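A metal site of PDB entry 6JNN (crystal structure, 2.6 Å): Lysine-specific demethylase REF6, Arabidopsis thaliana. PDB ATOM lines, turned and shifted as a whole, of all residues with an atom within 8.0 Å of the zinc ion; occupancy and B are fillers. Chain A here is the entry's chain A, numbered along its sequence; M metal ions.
CE1 of His 87 touches the zinc ion, 2.6 Å away. The nearest printed residue that does not touch the zinc ion is Gln 76 (4.05 Å).
The zinc ion is bound by a ring nitrogen (ND1) of His 93, the side-chain sulfur (SG) of Cys 69 and the side-chain sulfur (SG) of Cys 74.
The side-chain hydroxyl (OG1) of Thr 91 sits close to the backbone NH (N) of His 93. The backbone carbonyl oxygen (O) of Gln 76 lies within hydrogen-bond range of the backbone NH (N) of Cys 69, 3.2 Å away. SG of Cys 69 sits close to N of Glu 71, at 3.8 Å. NE2 of Gln 76 sits close to SG of Cys 74. A ring nitrogen (NE2) of His 87 sits at hydrogen-bond distance from the side-chain amide nitrogen (NE2) of Gln 76. The backbone carbonyl oxygen of His 87 lies within hydrogen-bond range of the side-chain hydroxyl of Thr 91.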
ATOM      1  N   VAL A  68     -13.377 -34.369  18.449  1.00  0.00           N
ATOM      2  CA  VAL A  68     -13.583 -33.106  17.736  1.00  0.00           C
ATOM      3  C   VAL A  68     -13.268 -31.966  18.672  1.00  0.00           C
ATOM      4  O   VAL A  68     -13.826 -31.879  19.771  1.00  0.00           O
ATOM      5  CB  VAL A  68     -15.043 -32.990  17.204  1.00  0.00           C
ATOM      6  CG1 VAL A  68     -15.277 -33.877  15.996  1.00  0.00           C
ATOM      7  CG2 VAL A  68     -16.078 -33.377  18.258  1.00  0.00           C
ATOM      8  N   CYS A  69     -12.343 -31.103  18.288  1.00  0.00           N
ATOM      9  CA  CYS A  69     -11.872 -30.035  19.180  1.00  0.00           C
ATOM     10  C   CYS A  69     -12.965 -29.023  19.441  1.00  0.00           C
ATOM     11  O   CYS A  69     -13.623 -28.536  18.474  1.00  0.00           O
ATOM     12  CB  CYS A  69     -10.640 -29.369  18.591  1.00  0.00           C
ATOM     13  SG  CYS A  69      -9.820 -28.294  19.757  1.00  0.00           S
ATOM     14  N   ALA A  70     -13.260 -28.770  20.737  1.00  0.00           N
ATOM     15  CA  ALA A  70     -14.372 -27.875  21.105  1.00  0.00           C
ATOM     16  C   ALA A  70     -13.973 -26.397  21.116  1.00  0.00           C
ATOM     17  O   ALA A  70     -14.807 -25.507  21.292  1.00  0.00           O
ATOM     18  CB  ALA A  70     -15.010 -28.295  22.418  1.00  0.00           C
ATOM     19  N   GLU A  71     -12.689 -26.135  20.935  1.00  0.00           N
ATOM     20  CA  GLU A  71     -12.108 -24.802  20.964  1.00  0.00           C
ATOM     21  C   GLU A  71     -12.420 -24.031  19.689  1.00  0.00           C
ATOM     22  O   GLU A  71     -12.225 -24.564  18.590  1.00  0.00           O
ATOM     23  CB  GLU A  71     -10.592 -24.923  21.133  1.00  0.00           C
ATOM     24  CG  GLU A  71      -9.848 -23.606  21.268  1.00  0.00           C
ATOM     25  CD  GLU A  71     -10.057 -22.967  22.655  1.00  0.00           C
ATOM     26  OE1 GLU A  71     -10.883 -23.446  23.453  1.00  0.00           O
ATOM     27  OE2 GLU A  71      -9.334 -22.007  22.997  1.00  0.00           O
ATOM     28  N   PRO A  72     -12.940 -22.796  19.822  1.00  0.00           N
ATOM     29  CA  PRO A  72     -13.287 -21.994  18.621  1.00  0.00           C
ATOM     30  C   PRO A  72     -12.047 -21.709  17.750  1.00  0.00           C
ATOM     31  O   PRO A  72     -10.959 -21.479  18.278  1.00  0.00           O
ATOM     32  CB  PRO A  72     -13.843 -20.687  19.199  1.00  0.00           C
ATOM     33  CG  PRO A  72     -13.696 -20.751  20.672  1.00  0.00           C
ATOM     34  CD  PRO A  72     -12.864 -21.937  21.012  1.00  0.00           C
ATOM     35  N   ASP A  73     -12.236 -21.770  16.435  1.00  0.00           N
ATOM     36  CA  ASP A  73     -11.158 -21.620  15.452  1.00  0.00           C
ATOM     37  C   ASP A  73     -10.077 -22.689  15.612  1.00  0.00           C
ATOM     38  O   ASP A  73      -8.886 -22.437  15.336  1.00  0.00           O
ATOM     39  CB  ASP A  73     -10.538 -20.213  15.446  1.00  0.00           C
ATOM     40  CG  ASP A  73     -11.515 -19.129  15.037  1.00  0.00           C
ATOM     41  OD1 ASP A  73     -11.815 -18.978  13.829  1.00  0.00           O
ATOM     42  OD2 ASP A  73     -11.976 -18.397  15.941  1.00  0.00           O
ATOM     43  N   CYS A  74     -10.470 -23.891  16.023  1.00  0.00           N
ATOM     44  CA  CYS A  74      -9.598 -25.052  15.880  1.00  0.00           C
ATOM     45  C   CYS A  74     -10.207 -26.031  14.863  1.00  0.00           C
ATOM     46  O   CYS A  74      -9.912 -25.967  13.680  1.00  0.00           O
ATOM     47  CB  CYS A  74      -9.256 -25.721  17.206  1.00  0.00           C
ATOM     48  SG  CYS A  74      -8.112 -27.067  16.983  1.00  0.00           S
ATOM     49  N   GLY A  75     -11.051 -26.924  15.340  1.00  0.00           N
ATOM     50  CA  GLY A  75     -11.751 -27.875  14.497  1.00  0.00           C
ATOM     51  C   GLY A  75     -10.868 -28.882  13.775  1.00  0.00           C
ATOM     52  O   GLY A  75     -11.235 -29.293  12.677  1.00  0.00           O
ATOM     53  N   GLN A  76      -9.803 -29.365  14.390  1.00  0.00           N
ATOM     54  CA  GLN A  76      -9.206 -30.638  13.966  1.00  0.00           C
ATOM     55  C   GLN A  76      -9.979 -31.775  14.610  1.00  0.00           C
ATOM     56  O   GLN A  76     -10.735 -31.584  15.569  1.00  0.00           O
ATOM     57  CB  GLN A  76      -7.749 -30.751  14.358  1.00  0.00           C
ATOM     58  CG  GLN A  76      -6.801 -29.755  13.770  1.00  0.00           C
ATOM     59  CD  GLN A  76      -5.772 -29.329  14.797  1.00  0.00           C
ATOM     60  OE1 GLN A  76      -4.692 -29.935  14.913  1.00  0.00           O
ATOM     61  NE2 GLN A  76      -6.108 -28.298  15.563  1.00  0.00           N
ATOM     62  N   THR A  77      -9.816 -32.962  14.051  1.00  0.00           N
ATOM     63  CA  THR A  77     -10.414 -34.168  14.566  1.00  0.00           C
ATOM     64  C   THR A  77      -9.376 -35.250  14.754  1.00  0.00           C
ATOM     65  O   THR A  77      -8.294 -35.152  14.153  1.00  0.00           O
ATOM     66  CB  THR A  77     -11.543 -34.705  13.691  1.00  0.00           C
ATOM     67  OG1 THR A  77     -10.979 -35.212  12.490  1.00  0.00           O
ATOM     68  CG2 THR A  77     -12.531 -33.599  13.334  1.00  0.00           C
ATOM     69  N   PHE A  78      -9.652 -36.237  15.616  1.00  0.00           N
ATOM     70  CA  PHE A  78      -8.708 -37.339  15.838  1.00  0.00           C
ATOM     71  C   PHE A  78      -9.377 -38.682  15.963  1.00  0.00           C
ATOM     72  O   PHE A  78     -10.441 -38.790  16.554  1.00  0.00           O
ATOM     73  CB  PHE A  78      -7.842 -37.059  17.070  1.00  0.00           C
ATOM     74  CG  PHE A  78      -7.245 -35.714  17.084  1.00  0.00           C
ATOM     75  CD1 PHE A  78      -7.910 -34.615  17.603  1.00  0.00           C
ATOM     76  CD2 PHE A  78      -5.957 -35.558  16.619  1.00  0.00           C
ATOM     77  CE1 PHE A  78      -7.362 -33.373  17.575  1.00  0.00           C
ATOM     78  CE2 PHE A  78      -5.336 -34.317  16.638  1.00  0.00           C
ATOM     79  CZ  PHE A  78      -6.048 -33.229  17.118  1.00  0.00           C
ATOM     80  N   PHE A  84      -5.526 -36.826  20.615  1.00  0.00           N
ATOM     81  CA  PHE A  84      -6.254 -35.682  21.190  1.00  0.00           C
ATOM     82  C   PHE A  84      -5.633 -35.165  22.489  1.00  0.00           C
ATOM     83  O   PHE A  84      -5.610 -33.949  22.736  1.00  0.00           O
ATOM     84  CB  PHE A  84      -7.716 -36.012  21.409  1.00  0.00           C
ATOM     85  CG  PHE A  84      -8.595 -34.811  21.749  1.00  0.00           C
ATOM     86  CD1 PHE A  84      -8.372 -33.530  21.214  1.00  0.00           C
ATOM     87  CD2 PHE A  84      -9.755 -35.005  22.528  1.00  0.00           C
ATOM     88  CE1 PHE A  84      -9.212 -32.466  21.513  1.00  0.00           C
ATOM     89  CE2 PHE A  84     -10.625 -33.947  22.805  1.00  0.00           C
ATOM     90  CZ  PHE A  84     -10.360 -32.672  22.295  1.00  0.00           C
ATOM     91  N   HIS A  87      -2.558 -33.396  21.787  1.00  0.00           N
ATOM     92  CA  HIS A  87      -2.974 -32.163  21.143  1.00  0.00           C
ATOM     93  C   HIS A  87      -3.267 -31.086  22.174  1.00  0.00           C
ATOM     94  O   HIS A  87      -2.654 -30.009  22.143  1.00  0.00           O
ATOM     95  CB  HIS A  87      -4.167 -32.399  20.250  1.00  0.00           C
ATOM     96  CG  HIS A  87      -4.748 -31.148  19.677  1.00  0.00           C
ATOM     97  ND1 HIS A  87      -5.748 -30.435  20.316  1.00  0.00           N
ATOM     98  CD2 HIS A  87      -4.506 -30.516  18.511  1.00  0.00           C
ATOM     99  CE1 HIS A  87      -6.071 -29.395  19.577  1.00  0.00           C
ATOM    100  NE2 HIS A  87      -5.333 -29.419  18.470  1.00  0.00           N
ATOM    101  N   LYS A  88      -4.223 -31.312  23.082  1.00  0.00           N
ATOM    102  CA  LYS A  88      -4.527 -30.246  24.060  1.00  0.00           C
ATOM    103  C   LYS A  88      -3.330 -30.002  24.964  1.00  0.00           C
ATOM    104  O   LYS A  88      -3.141 -28.916  25.404  1.00  0.00           O
ATOM    105  CB  LYS A  88      -5.828 -30.498  24.809  1.00  0.00           C
ATOM    106  CG  LYS A  88      -6.005 -31.824  25.481  1.00  0.00           C
ATOM    107  CD  LYS A  88      -7.449 -32.305  25.184  1.00  0.00           C
ATOM    108  CE  LYS A  88      -7.940 -33.378  26.151  1.00  0.00           C
ATOM    109  NZ  LYS A  88      -9.398 -33.638  26.064  1.00  0.00           N
ATOM    110  N   THR A  91      -1.453 -27.498  22.958  1.00  0.00           N
ATOM    111  CA  THR A  91      -2.245 -26.317  22.634  1.00  0.00           C
ATOM    112  C   THR A  91      -2.947 -25.652  23.844  1.00  0.00           C
ATOM    113  O   THR A  91      -3.105 -24.437  23.913  1.00  0.00           O
ATOM    114  CB  THR A  91      -3.259 -26.573  21.489  1.00  0.00           C
ATOM    115  OG1 THR A  91      -4.386 -27.354  21.938  1.00  0.00           O
ATOM    116  CG2 THR A  91      -2.649 -27.255  20.292  1.00  0.00           C
ATOM    117  N   GLY A  92      -3.401 -26.477  24.776  1.00  0.00           N
ATOM    118  CA  GLY A  92      -4.151 -26.036  25.943  1.00  0.00           C
ATOM    119  C   GLY A  92      -5.644 -25.844  25.701  1.00  0.00           C
ATOM    120  O   GLY A  92      -6.336 -25.220  26.538  1.00  0.00           O
ATOM    121  N   HIS A  93      -6.154 -26.466  24.644  1.00  0.00           N
ATOM    122  CA  HIS A  93      -7.597 -26.327  24.340  1.00  0.00           C
ATOM    123  C   HIS A  93      -8.452 -27.233  25.213  1.00  0.00           C
ATOM    124  O   HIS A  93      -8.088 -28.370  25.468  1.00  0.00           O
ATOM    125  CB  HIS A  93      -7.923 -26.614  22.897  1.00  0.00           C
ATOM    126  CG  HIS A  93      -7.164 -25.803  21.891  1.00  0.00           C
ATOM    127  ND1 HIS A  93      -7.248 -26.026  20.537  1.00  0.00           N
ATOM    128  CD2 HIS A  93      -6.318 -24.757  22.034  1.00  0.00           C
ATOM    129  CE1 HIS A  93      -6.472 -25.183  19.892  1.00  0.00           C
ATOM    130  NE2 HIS A  93      -5.882 -24.406  20.780  1.00  0.00           N
ATOM    131  N   SER A  94      -9.533 -26.658  25.729  1.00  0.00           N
ATOM    132  CA  SER A  94     -10.456 -27.349  26.680  1.00  0.00           C
ATOM    133  C   SER A  94      -9.773 -27.869  27.971  1.00  0.00           C
ATOM    134  O   SER A  94      -9.592 -27.153  28.939  1.00  0.00           O
ATOM    135  CB  SER A  94     -11.165 -28.538  25.995  1.00  0.00           C
ATOM    136  OG  SER A  94     -11.603 -28.212  24.689  1.00  0.00           O
HETATM  137 ZN    ZN M   1      -7.859 -27.520  19.131  1.00  0.00          ZN
